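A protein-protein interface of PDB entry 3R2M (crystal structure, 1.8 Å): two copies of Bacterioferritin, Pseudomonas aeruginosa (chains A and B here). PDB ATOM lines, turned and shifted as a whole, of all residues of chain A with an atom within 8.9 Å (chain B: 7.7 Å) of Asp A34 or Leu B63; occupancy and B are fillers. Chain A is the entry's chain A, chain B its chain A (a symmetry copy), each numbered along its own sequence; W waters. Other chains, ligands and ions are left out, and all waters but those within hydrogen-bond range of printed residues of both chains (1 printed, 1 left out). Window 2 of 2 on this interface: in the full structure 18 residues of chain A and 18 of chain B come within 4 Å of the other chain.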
ATOM      1  N   PHE A  26      -1.767  21.560 -20.527  1.00  0.00           N
ATOM      2  CA  PHE A  26      -1.878  21.632 -22.008  1.00  0.00           C
ATOM      3  C   PHE A  26      -0.538  21.152 -22.607  1.00  0.00           C
ATOM      4  O   PHE A  26      -0.472  20.193 -23.383  1.00  0.00           O
ATOM      5  CB  PHE A  26      -2.188  23.090 -22.438  1.00  0.00           C
ATOM      6  CG  PHE A  26      -2.798  23.263 -23.839  1.00  0.00           C
ATOM      7  CD1 PHE A  26      -2.933  22.205 -24.741  1.00  0.00           C
ATOM      8  CD2 PHE A  26      -3.222  24.525 -24.244  1.00  0.00           C
ATOM      9  CE1 PHE A  26      -3.487  22.404 -25.988  1.00  0.00           C
ATOM     10  CE2 PHE A  26      -3.785  24.737 -25.499  1.00  0.00           C
ATOM     11  CZ  PHE A  26      -3.937  23.665 -26.369  1.00  0.00           C
ATOM     12  N   ILE A  27       0.553  21.795 -22.223  1.00  0.00           N
ATOM     13  CA  ILE A  27       1.836  21.417 -22.795  1.00  0.00           C
ATOM     14  C   ILE A  27       2.275  20.028 -22.334  1.00  0.00           C
ATOM     15  O   ILE A  27       2.720  19.228 -23.177  1.00  0.00           O
ATOM     16  CB  ILE A  27       2.952  22.508 -22.552  1.00  0.00           C
ATOM     17  CG1 ILE A  27       4.283  22.078 -23.191  1.00  0.00           C
ATOM     18  CG2 ILE A  27       3.192  22.742 -21.038  1.00  0.00           C
ATOM     19  CD1 ILE A  27       4.237  21.886 -24.690  1.00  0.00           C
ATOM     20  N   HIS A  28       2.165  19.690 -21.045  1.00  0.00           N
ATOM     21  CA  HIS A  28       2.590  18.337 -20.629  1.00  0.00           C
ATOM     22  C   HIS A  28       1.798  17.210 -21.315  1.00  0.00           C
ATOM     23  O   HIS A  28       2.380  16.198 -21.722  1.00  0.00           O
ATOM     24  CB  HIS A  28       2.490  18.122 -19.115  1.00  0.00           C
ATOM     25  CG  HIS A  28       3.612  18.761 -18.333  1.00  0.00           C
ATOM     26  ND1 HIS A  28       3.541  18.948 -16.974  1.00  0.00           N
ATOM     27  CD2 HIS A  28       4.822  19.245 -18.724  1.00  0.00           C
ATOM     28  CE1 HIS A  28       4.670  19.514 -16.546  1.00  0.00           C
ATOM     29  NE2 HIS A  28       5.456  19.711 -17.589  1.00  0.00           N
ATOM     30  N   SER A  29       0.477  17.344 -21.415  1.00  0.00           N
ATOM     31  CA  SER A  29      -0.303  16.280 -22.051  1.00  0.00           C
ATOM     32  C   SER A  29       0.138  16.051 -23.493  1.00  0.00           C
ATOM     33  O   SER A  29       0.297  14.885 -23.931  1.00  0.00           O
ATOM     34  CB  SER A  29      -1.810  16.564 -21.966  1.00  0.00           C
ATOM     35  OG  SER A  29      -2.125  17.784 -22.593  1.00  0.00           O
ATOM     36  N   ARG A  30       0.413  17.145 -24.217  1.00  0.00           N
ATOM     37  CA  ARG A  30       0.808  17.018 -25.608  1.00  0.00           C
ATOM     38  C   ARG A  30       2.235  16.489 -25.742  1.00  0.00           C
ATOM     39  O   ARG A  30       2.543  15.776 -26.704  1.00  0.00           O
ATOM     40  CB  ARG A  30       0.604  18.327 -26.368  1.00  0.00           C
ATOM     41  CG  ARG A  30      -0.807  18.495 -26.960  1.00  0.00           C
ATOM     42  CD  ARG A  30      -1.909  18.513 -25.866  1.00  0.00           C
ATOM     43  NE  ARG A  30      -3.248  18.761 -26.435  1.00  0.00           N
ATOM     44  CZ  ARG A  30      -4.384  18.611 -25.758  1.00  0.00           C
ATOM     45  NH1 ARG A  30      -4.348  18.203 -24.484  1.00  0.00           N
ATOM     46  NH2 ARG A  30      -5.549  18.852 -26.347  1.00  0.00           N
ATOM     47  N   MET A  31       3.107  16.794 -24.783  1.00  0.00           N
ATOM     48  CA  MET A  31       4.454  16.205 -24.784  1.00  0.00           C
ATOM     49  C   MET A  31       4.373  14.700 -24.550  1.00  0.00           C
ATOM     50  O   MET A  31       5.080  13.944 -25.181  1.00  0.00           O
ATOM     51  CB  MET A  31       5.315  16.836 -23.667  1.00  0.00           C
ATOM     52  CG  MET A  31       5.745  18.283 -23.994  1.00  0.00           C
ATOM     53  SD  MET A  31       6.507  19.091 -22.568  1.00  0.00           S
ATOM     54  CE  MET A  31       7.929  18.052 -22.309  1.00  0.00           C
ATOM     55  N   TYR A  32       3.514  14.281 -23.629  1.00  0.00           N
ATOM     56  CA  TYR A  32       3.348  12.871 -23.322  1.00  0.00           C
ATOM     57  C   TYR A  32       2.891  12.144 -24.581  1.00  0.00           C
ATOM     58  O   TYR A  32       3.337  11.035 -24.851  1.00  0.00           O
ATOM     59  CB  TYR A  32       2.303  12.652 -22.214  1.00  0.00           C
ATOM     60  CG  TYR A  32       2.750  13.012 -20.811  1.00  0.00           C
ATOM     61  CD1 TYR A  32       3.995  12.597 -20.333  1.00  0.00           C
ATOM     62  CD2 TYR A  32       1.912  13.687 -19.948  1.00  0.00           C
ATOM     63  CE1 TYR A  32       4.410  12.897 -19.033  1.00  0.00           C
ATOM     64  CE2 TYR A  32       2.318  13.985 -18.611  1.00  0.00           C
ATOM     65  CZ  TYR A  32       3.573  13.586 -18.183  1.00  0.00           C
ATOM     66  OH  TYR A  32       3.997  13.852 -16.904  1.00  0.00           O
ATOM     67  N   GLU A  33       2.004  12.762 -25.353  1.00  0.00           N
ATOM     68  CA  GLU A  33       1.513  12.113 -26.576  1.00  0.00           C
ATOM     69  C   GLU A  33       2.597  12.087 -27.664  1.00  0.00           C
ATOM     70  O   GLU A  33       2.692  11.128 -28.420  1.00  0.00           O
ATOM     71  CB  GLU A  33       0.241  12.796 -27.097  1.00  0.00           C
ATOM     72  CG  GLU A  33      -0.293  12.183 -28.397  1.00  0.00           C
ATOM     73  CD  GLU A  33      -0.754  10.721 -28.259  1.00  0.00           C
ATOM     74  OE1 GLU A  33      -0.866  10.040 -29.311  1.00  0.00           O
ATOM     75  OE2 GLU A  33      -1.020  10.250 -27.122  1.00  0.00           O
ATOM     76  N   ASP A  34       3.419  13.126 -27.724  1.00  0.00           N
ATOM     77  CA  ASP A  34       4.539  13.213 -28.678  1.00  0.00           C
ATOM     78  C   ASP A  34       5.518  12.045 -28.440  1.00  0.00           C
ATOM     79  O   ASP A  34       6.094  11.505 -29.389  1.00  0.00           O
ATOM     80  CB  ASP A  34       5.204  14.605 -28.543  1.00  0.00           C
ATOM     81  CG  ASP A  34       6.559  14.727 -29.285  1.00  0.00           C
ATOM     82  OD1 ASP A  34       6.569  14.570 -30.519  1.00  0.00           O
ATOM     83  OD2 ASP A  34       7.597  15.063 -28.625  1.00  0.00           O
ATOM     84  N   TRP A  35       5.663  11.614 -27.188  1.00  0.00           N
ATOM     85  CA  TRP A  35       6.542  10.489 -26.873  1.00  0.00           C
ATOM     86  C   TRP A  35       5.844   9.117 -26.941  1.00  0.00           C
ATOM     87  O   TRP A  35       6.479   8.098 -26.712  1.00  0.00           O
ATOM     88  CB  TRP A  35       7.147  10.670 -25.470  1.00  0.00           C
ATOM     89  CG  TRP A  35       8.074  11.867 -25.316  1.00  0.00           C
ATOM     90  CD1 TRP A  35       8.852  12.442 -26.278  1.00  0.00           C
ATOM     91  CD2 TRP A  35       8.307  12.609 -24.114  1.00  0.00           C
ATOM     92  NE1 TRP A  35       9.547  13.513 -25.750  1.00  0.00           N
ATOM     93  CE2 TRP A  35       9.243  13.619 -24.420  1.00  0.00           C
ATOM     94  CE3 TRP A  35       7.825  12.506 -22.804  1.00  0.00           C
ATOM     95  CZ2 TRP A  35       9.683  14.535 -23.474  1.00  0.00           C
ATOM     96  CZ3 TRP A  35       8.268  13.419 -21.867  1.00  0.00           C
ATOM     97  CH2 TRP A  35       9.177  14.424 -22.208  1.00  0.00           C
ATOM     98  N   GLY A  36       4.544   9.081 -27.226  1.00  0.00           N
ATOM     99  CA  GLY A  36       3.836   7.810 -27.296  1.00  0.00           C
ATOM    100  C   GLY A  36       3.230   7.277 -25.999  1.00  0.00           C
ATOM    101  O   GLY A  36       2.854   6.099 -25.948  1.00  0.00           O
ATOM    102  N   PHE A  37       3.121   8.102 -24.954  1.00  0.00           N
ATOM    103  CA  PHE A  37       2.488   7.665 -23.696  1.00  0.00           C
ATOM    104  C   PHE A  37       1.031   8.110 -23.676  1.00  0.00           C
ATOM    105  O   PHE A  37       0.697   9.142 -23.083  1.00  0.00           O
ATOM    106  CB  PHE A  37       3.232   8.258 -22.478  1.00  0.00           C
ATOM    107  CG  PHE A  37       4.679   7.797 -22.399  1.00  0.00           C
ATOM    108  CD1 PHE A  37       4.972   6.452 -22.258  1.00  0.00           C
ATOM    109  CD2 PHE A  37       5.718   8.703 -22.516  1.00  0.00           C
ATOM    110  CE1 PHE A  37       6.292   6.027 -22.240  1.00  0.00           C
ATOM    111  CE2 PHE A  37       7.037   8.279 -22.477  1.00  0.00           C
ATOM    112  CZ  PHE A  37       7.310   6.955 -22.337  1.00  0.00           C
ATOM    113  N   SER A  38       0.152   7.362 -24.337  1.00  0.00           N
ATOM    114  CA  SER A  38      -1.205   7.867 -24.503  1.00  0.00           C
ATOM    115  C   SER A  38      -2.012   7.877 -23.203  1.00  0.00           C
ATOM    116  O   SER A  38      -2.944   8.669 -23.071  1.00  0.00           O
ATOM    117  CB  SER A  38      -1.920   7.120 -25.627  1.00  0.00           C
ATOM    118  OG  SER A  38      -1.359   7.531 -26.864  1.00  0.00           O
ATOM    119  N   LEU A  40      -0.874   8.813 -20.315  1.00  0.00           N
ATOM    120  CA  LEU A  40      -0.500  10.081 -19.648  1.00  0.00           C
ATOM    121  C   LEU A  40      -1.127  11.264 -20.397  1.00  0.00           C
ATOM    122  O   LEU A  40      -1.607  12.238 -19.770  1.00  0.00           O
ATOM    123  CB  LEU A  40       1.043  10.221 -19.537  1.00  0.00           C
ATOM    124  CG  LEU A  40       1.657   9.274 -18.515  1.00  0.00           C
ATOM    125  CD1 LEU A  40       3.189   9.314 -18.586  1.00  0.00           C
ATOM    126  CD2 LEU A  40       1.203   9.624 -17.071  1.00  0.00           C
ATOM    127  N   TYR A  41      -1.157  11.194 -21.724  1.00  0.00           N
ATOM    128  CA  TYR A  41      -1.851  12.233 -22.502  1.00  0.00           C
ATOM    129  C   TYR A  41      -3.299  12.327 -22.020  1.00  0.00           C
ATOM    130  O   TYR A  41      -3.807  13.423 -21.769  1.00  0.00           O
ATOM    131  CB  TYR A  41      -1.863  11.922 -24.016  1.00  0.00           C
ATOM    132  CG  TYR A  41      -2.906  12.730 -24.731  1.00  0.00           C
ATOM    133  CD1 TYR A  41      -4.164  12.188 -25.021  1.00  0.00           C
ATOM    134  CD2 TYR A  41      -2.654  14.040 -25.111  1.00  0.00           C
ATOM    135  CE1 TYR A  41      -5.152  12.953 -25.644  1.00  0.00           C
ATOM    136  CE2 TYR A  41      -3.631  14.812 -25.739  1.00  0.00           C
ATOM    137  CZ  TYR A  41      -4.873  14.253 -26.007  1.00  0.00           C
ATOM    138  OH  TYR A  41      -5.821  15.024 -26.626  1.00  0.00           O
ATOM    139  N   MET A  85       8.252  16.169 -15.202  1.00  0.00           N
ATOM    140  CA  MET A  85       6.927  16.741 -15.481  1.00  0.00           C
ATOM    141  C   MET A  85       5.915  16.408 -14.360  1.00  0.00           C
ATOM    142  O   MET A  85       5.123  17.266 -13.937  1.00  0.00           O
ATOM    143  CB  MET A  85       6.422  16.230 -16.843  1.00  0.00           C
ATOM    144  CG  MET A  85       7.283  16.685 -18.023  1.00  0.00           C
ATOM    145  SD  MET A  85       7.193  15.570 -19.437  1.00  0.00           S
ATOM    146  CE  MET A  85       5.565  15.986 -20.063  1.00  0.00           C
ATOM    147  N   MET B   1      11.410  14.416 -36.957  1.00  0.00           N
ATOM    148  CA  MET B   1      11.933  15.248 -38.091  1.00  0.00           C
ATOM    149  C   MET B   1      12.108  16.672 -37.583  1.00  0.00           C
ATOM    150  O   MET B   1      11.190  17.230 -36.992  1.00  0.00           O
ATOM    151  CB  MET B   1      10.928  15.223 -39.261  1.00  0.00           C
ATOM    152  CG  MET B   1      11.311  16.048 -40.497  1.00  0.00           C
ATOM    153  SD  MET B   1       9.991  16.156 -41.779  1.00  0.00           S
ATOM    154  CE  MET B   1       8.673  17.078 -40.968  1.00  0.00           C
ATOM    155  N   ILE B   8       9.603  26.966 -37.183  1.00  0.00           N
ATOM    156  CA  ILE B   8       9.263  26.658 -35.800  1.00  0.00           C
ATOM    157  C   ILE B   8       9.070  27.944 -35.008  1.00  0.00           C
ATOM    158  O   ILE B   8       8.089  28.088 -34.283  1.00  0.00           O
ATOM    159  CB  ILE B   8      10.311  25.707 -35.147  1.00  0.00           C
ATOM    160  CG1 ILE B   8      10.262  24.320 -35.806  1.00  0.00           C
ATOM    161  CG2 ILE B   8      10.096  25.597 -33.641  1.00  0.00           C
ATOM    162  CD1 ILE B   8      11.442  23.423 -35.444  1.00  0.00           C
ATOM    163  N   LEU B  11       5.720  29.471 -36.041  1.00  0.00           N
ATOM    164  CA  LEU B  11       4.581  28.701 -35.480  1.00  0.00           C
ATOM    165  C   LEU B  11       4.409  29.096 -34.016  1.00  0.00           C
ATOM    166  O   LEU B  11       3.299  29.244 -33.540  1.00  0.00           O
ATOM    167  CB  LEU B  11       4.819  27.185 -35.601  1.00  0.00           C
ATOM    168  CG  LEU B  11       4.846  26.651 -37.045  1.00  0.00           C
ATOM    169  CD1 LEU B  11       5.018  25.151 -37.024  1.00  0.00           C
ATOM    170  CD2 LEU B  11       3.572  27.093 -37.845  1.00  0.00           C
ATOM    171  N   ASN B  12       5.516  29.272 -33.294  1.00  0.00           N
ATOM    172  CA  ASN B  12       5.455  29.684 -31.891  1.00  0.00           C
ATOM    173  C   ASN B  12       4.821  31.060 -31.723  1.00  0.00           C
ATOM    174  O   ASN B  12       4.064  31.283 -30.785  1.00  0.00           O
ATOM    175  CB  ASN B  12       6.853  29.662 -31.263  1.00  0.00           C
ATOM    176  CG  ASN B  12       7.113  28.384 -30.518  1.00  0.00           C
ATOM    177  OD1 ASN B  12       6.180  27.805 -29.964  1.00  0.00           O
ATOM    178  ND2 ASN B  12       8.379  27.948 -30.457  1.00  0.00           N
ATOM    179  N   ASP B  56      -4.026  24.084 -30.188  1.00  0.00           N
ATOM    180  CA  ASP B  56      -3.628  22.684 -30.079  1.00  0.00           C
ATOM    181  C   ASP B  56      -2.961  22.216 -31.377  1.00  0.00           C
ATOM    182  O   ASP B  56      -1.937  21.528 -31.330  1.00  0.00           O
ATOM    183  CB  ASP B  56      -4.867  21.830 -29.777  1.00  0.00           C
ATOM    184  CG  ASP B  56      -4.539  20.418 -29.280  1.00  0.00           C
ATOM    185  OD1 ASP B  56      -3.416  20.117 -28.898  1.00  0.00           O
ATOM    186  OD2 ASP B  56      -5.485  19.598 -29.224  1.00  0.00           O
ATOM    187  N   ALA B  57      -3.561  22.506 -32.534  1.00  0.00           N
ATOM    188  CA  ALA B  57      -2.933  22.076 -33.810  1.00  0.00           C
ATOM    189  C   ALA B  57      -1.486  22.622 -33.952  1.00  0.00           C
ATOM    190  O   ALA B  57      -0.576  21.897 -34.364  1.00  0.00           O
ATOM    191  CB  ALA B  57      -3.767  22.507 -35.001  1.00  0.00           C
ATOM    192  N   LEU B  58      -1.279  23.896 -33.631  1.00  0.00           N
ATOM    193  CA  LEU B  58       0.067  24.487 -33.719  1.00  0.00           C
ATOM    194  C   LEU B  58       1.022  23.877 -32.721  1.00  0.00           C
ATOM    195  O   LEU B  58       2.164  23.542 -33.063  1.00  0.00           O
ATOM    196  CB  LEU B  58       0.009  26.001 -33.468  1.00  0.00           C
ATOM    197  CG  LEU B  58      -0.829  26.777 -34.482  1.00  0.00           C
ATOM    198  CD1 LEU B  58      -1.087  28.216 -34.010  1.00  0.00           C
ATOM    199  CD2 LEU B  58      -0.198  26.803 -35.859  1.00  0.00           C
ATOM    200  N   LEU B  59       0.565  23.725 -31.479  1.00  0.00           N
ATOM    201  CA  LEU B  59       1.391  23.104 -30.435  1.00  0.00           C
ATOM    202  C   LEU B  59       1.861  21.711 -30.858  1.00  0.00           C
ATOM    203  O   LEU B  59       3.044  21.390 -30.749  1.00  0.00           O
ATOM    204  CB  LEU B  59       0.590  23.022 -29.136  1.00  0.00           C
ATOM    205  CG  LEU B  59       1.341  22.685 -27.847  1.00  0.00           C
ATOM    206  CD1 LEU B  59       0.360  23.005 -26.695  1.00  0.00           C
ATOM    207  CD2 LEU B  59       1.771  21.264 -27.786  1.00  0.00           C
ATOM    208  N   ARG B  60       0.943  20.855 -31.322  1.00  0.00           N
ATOM    209  CA  ARG B  60       1.331  19.508 -31.743  1.00  0.00           C
ATOM    210  C   ARG B  60       2.283  19.509 -32.940  1.00  0.00           C
ATOM    211  O   ARG B  60       3.166  18.672 -33.010  1.00  0.00           O
ATOM    212  CB  ARG B  60       0.095  18.683 -32.111  1.00  0.00           C
ATOM    213  CG  ARG B  60      -0.825  18.485 -30.868  1.00  0.00           C
ATOM    214  CD  ARG B  60      -1.876  17.437 -31.124  1.00  0.00           C
ATOM    215  NE  ARG B  60      -2.988  17.546 -30.189  1.00  0.00           N
ATOM    216  CZ  ARG B  60      -3.604  16.517 -29.617  1.00  0.00           C
ATOM    217  NH1 ARG B  60      -3.199  15.296 -29.861  1.00  0.00           N
ATOM    218  NH2 ARG B  60      -4.637  16.712 -28.803  1.00  0.00           N
ATOM    219  N   ARG B  61       2.114  20.443 -33.864  1.00  0.00           N
ATOM    220  CA  ARG B  61       2.973  20.503 -35.046  1.00  0.00           C
ATOM    221  C   ARG B  61       4.399  20.929 -34.645  1.00  0.00           C
ATOM    222  O   ARG B  61       5.374  20.360 -35.119  1.00  0.00           O
ATOM    223  CB  ARG B  61       2.393  21.497 -36.055  1.00  0.00           C
ATOM    224  CG  ARG B  61       3.248  21.662 -37.321  1.00  0.00           C
ATOM    225  CD  ARG B  61       3.318  20.363 -38.121  1.00  0.00           C
ATOM    226  NE  ARG B  61       4.069  20.546 -39.368  1.00  0.00           N
ATOM    227  CZ  ARG B  61       4.475  19.559 -40.149  1.00  0.00           C
ATOM    228  NH1 ARG B  61       4.157  18.283 -39.857  1.00  0.00           N
ATOM    229  NH2 ARG B  61       5.194  19.847 -41.230  1.00  0.00           N
ATOM    230  N   ILE B  62       4.496  21.889 -33.737  1.00  0.00           N
ATOM    231  CA  ILE B  62       5.792  22.318 -33.181  1.00  0.00           C
ATOM    232  C   ILE B  62       6.506  21.147 -32.511  1.00  0.00           C
ATOM    233  O   ILE B  62       7.708  20.922 -32.756  1.00  0.00           O
ATOM    234  CB  ILE B  62       5.591  23.470 -32.198  1.00  0.00           C
ATOM    235  CG1 ILE B  62       5.207  24.743 -32.950  1.00  0.00           C
ATOM    236  CG2 ILE B  62       6.868  23.767 -31.381  1.00  0.00           C
ATOM    237  CD1 ILE B  62       4.400  25.729 -32.069  1.00  0.00           C
ATOM    238  N   LEU B  63       5.791  20.371 -31.682  1.00  0.00           N
ATOM    239  CA  LEU B  63       6.403  19.191 -31.051  1.00  0.00           C
ATOM    240  C   LEU B  63       6.836  18.173 -32.108  1.00  0.00           C
ATOM    241  O   LEU B  63       7.921  17.602 -32.021  1.00  0.00           O
ATOM    242  CB  LEU B  63       5.430  18.518 -30.059  1.00  0.00           C
ATOM    243  CG  LEU B  63       5.200  19.318 -28.770  1.00  0.00           C
ATOM    244  CD1 LEU B  63       4.082  18.681 -27.939  1.00  0.00           C
ATOM    245  CD2 LEU B  63       6.549  19.430 -27.926  1.00  0.00           C
ATOM    246  N   LEU B  64       5.981  17.913 -33.106  1.00  0.00           N
ATOM    247  CA  LEU B  64       6.332  16.927 -34.148  1.00  0.00           C
ATOM    248  C   LEU B  64       7.660  17.322 -34.839  1.00  0.00           C
ATOM    249  O   LEU B  64       8.481  16.465 -35.235  1.00  0.00           O
ATOM    250  CB  LEU B  64       5.208  16.827 -35.188  1.00  0.00           C
ATOM    251  CG  LEU B  64       5.450  15.876 -36.373  1.00  0.00           C
ATOM    252  CD1 LEU B  64       4.116  15.396 -36.961  1.00  0.00           C
ATOM    253  CD2 LEU B  64       6.280  16.565 -37.439  1.00  0.00           C
ATOM    254  N   LEU B  65       7.845  18.633 -34.982  1.00  0.00           N
ATOM    255  CA  LEU B  65       8.994  19.215 -35.694  1.00  0.00           C
ATOM    256  C   LEU B  65      10.176  19.387 -34.743  1.00  0.00           C
ATOM    257  O   LEU B  65      11.192  20.012 -35.099  1.00  0.00           O
ATOM    258  CB  LEU B  65       8.619  20.584 -36.273  1.00  0.00           C
ATOM    259  CG  LEU B  65       7.590  20.579 -37.419  1.00  0.00           C
ATOM    260  CD1 LEU B  65       7.320  21.992 -37.909  1.00  0.00           C
ATOM    261  CD2 LEU B  65       8.059  19.697 -38.529  1.00  0.00           C
ATOM    262  N   GLU B  66      10.022  18.833 -33.538  1.00  0.00           N
ATOM    263  CA  GLU B  66      11.085  18.768 -32.530  1.00  0.00           C
ATOM    264  C   GLU B  66      11.430  20.126 -31.942  1.00  0.00           C
ATOM    265  O   GLU B  66      12.541  20.350 -31.427  1.00  0.00           O
ATOM    266  CB  GLU B  66      12.314  18.062 -33.110  1.00  0.00           C
ATOM    267  CG  GLU B  66      11.936  16.683 -33.624  1.00  0.00           C
ATOM    268  CD  GLU B  66      13.108  15.792 -33.924  1.00  0.00           C
ATOM    269  OE1 GLU B  66      14.185  16.018 -33.357  1.00  0.00           O
ATOM    270  OE2 GLU B  66      12.949  14.866 -34.745  1.00  0.00           O
ATOM    271  N   GLY B  67      10.460  21.032 -31.987  1.00  0.00           N
ATOM    272  CA  GLY B  67      10.610  22.342 -31.373  1.00  0.00           C
ATOM    273  C   GLY B  67      10.044  22.350 -29.968  1.00  0.00           C
ATOM    274  O   GLY B  67       9.464  21.357 -29.514  1.00  0.00           O
ATOM    275  N   THR B  68      10.212  23.469 -29.273  1.00  0.00           N
ATOM    276  CA  THR B  68       9.715  23.618 -27.904  1.00  0.00           C
ATOM    277  C   THR B  68       8.613  24.669 -27.881  1.00  0.00           C
ATOM    278  O   THR B  68       8.857  25.830 -28.221  1.00  0.00           O
ATOM    279  CB  THR B  68      10.844  24.076 -26.963  1.00  0.00           C
ATOM    280  OG1 THR B  68      11.922  23.135 -27.017  1.00  0.00           O
ATOM    281  CG2 THR B  68      10.332  24.215 -25.524  1.00  0.00           C
ATOM    282  N   PRO B  69       7.374  24.280 -27.519  1.00  0.00           N
ATOM    283  CA  PRO B  69       6.334  25.306 -27.674  1.00  0.00           C
ATOM    284  C   PRO B  69       6.427  26.446 -26.644  1.00  0.00           C
ATOM    285  O   PRO B  69       6.814  26.251 -25.493  1.00  0.00           O
ATOM    286  CB  PRO B  69       5.010  24.506 -27.517  1.00  0.00           C
ATOM    287  CG  PRO B  69       5.390  23.089 -27.881  1.00  0.00           C
ATOM    288  CD  PRO B  69       6.799  22.925 -27.341  1.00  0.00           C
HETATM  289  O   HOH W   1       9.247  16.911 -29.656  1.00  0.00           O
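NE of Arg A30 is in salt-bridge range of OD1 of Asp B56 (2.8 Å). NH2 of Arg B60 lies within hydrogen-bond range of OH of Tyr A41 (3.0 Å). NH2 of Arg A30 sits close to NH2 of Arg B60 (3.4 Å).
The backbone carbonyl oxygen (O) of Phe A26 sits at hydrogen-bond distance from the side-chain hydroxyl (OG) of Ser A29 (3.0 Å). OG of Ser A29 sits at hydrogen-bond distance from NH1 of Arg A30 (2.9 Å). The side-chain carboxylate (OD1) of Asp B56 is in salt-bridge range of the guanidinium group (NE) of Arg B60 (2.9 Å).
Phe A26 touches Asp B56 (CE1 to OD1, 3.7 Å). CD1 of Leu B59 touches CD1 of Phe A26, at 3.9 Å. CD1 of Ile A27 touches CG of Pro B69 (3.6 Å). CB of Arg A30 touches CD2 of Leu B59 (3.5 Å). O of Arg A30 touches CD1 of Leu B63, at 3.5 Å. Met A31 touches Leu B63 (N to CD1, 3.8 Å). Asp A34 touches Leu B63.
Of the printed residues of chain B, Asp A34 touches Leu B63. Of the printed residues of chain A, Leu B63 touches Arg A30 (3.5 Å), Met A31 (3.8 Å) and Asp A34 (3.6 Å). Of the printed residues of chain B, Ile A27 touches Pro B69 (3.6 Å). Of the printed residues of chain B, Phe A26 touches Asp B56 and Leu B59. Printed residues of chain B within 4 Å of Arg A30: Asp B56 (2.8 Å), Leu B59 (3.5 Å), Arg B60 (3.4 Å) and Leu B63 (3.5 Å). Of the printed residues of chain A, Asp B56 touches Phe A26 (3.7 Å) and Arg A30 (2.8 Å). Printed residues of chain B within 4 Å of Met A31: Leu B63. The nearest residue of chain A that does not touch Leu B63 is Ile A27 (4.6 Å).
Printed residues of chain B that touch a printed residue of chain A: Asp B56, Leu B59, Arg B60, Leu B63 and Pro B69. Along chain B the printed residues that touch a printed residue of chain A span positions 56 to 69. Of the 16 printed residues of chain A, 6 touch a printed residue of chain B. Printed residues of chain A that touch a printed residue of chain B: Phe A26, Ile A27, Arg A30, Met A31, Asp A34 and Tyr A41. Hydrophobic or aromatic side chains of chain A within 4 Å of the printed part of chain B: Phe A26, Ile A27 and Tyr A41. Along chain A the printed residues that touch a printed residue of chain B span positions 26 to 41. Among the printed residues, Asp or Glu carboxylates within 4 Å of a Lys or Arg side-chain nitrogen of the other chain: Arg A30 with Asp B56 (2.8 Å).
No position is printed for both chains.
Water W1 lies within hydrogen-bond range of the side-chain carboxylate (OD2) of Asp A34 (2.7 Å) and the backbone carbonyl oxygen (O) of Leu B63 (2.8 Å).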
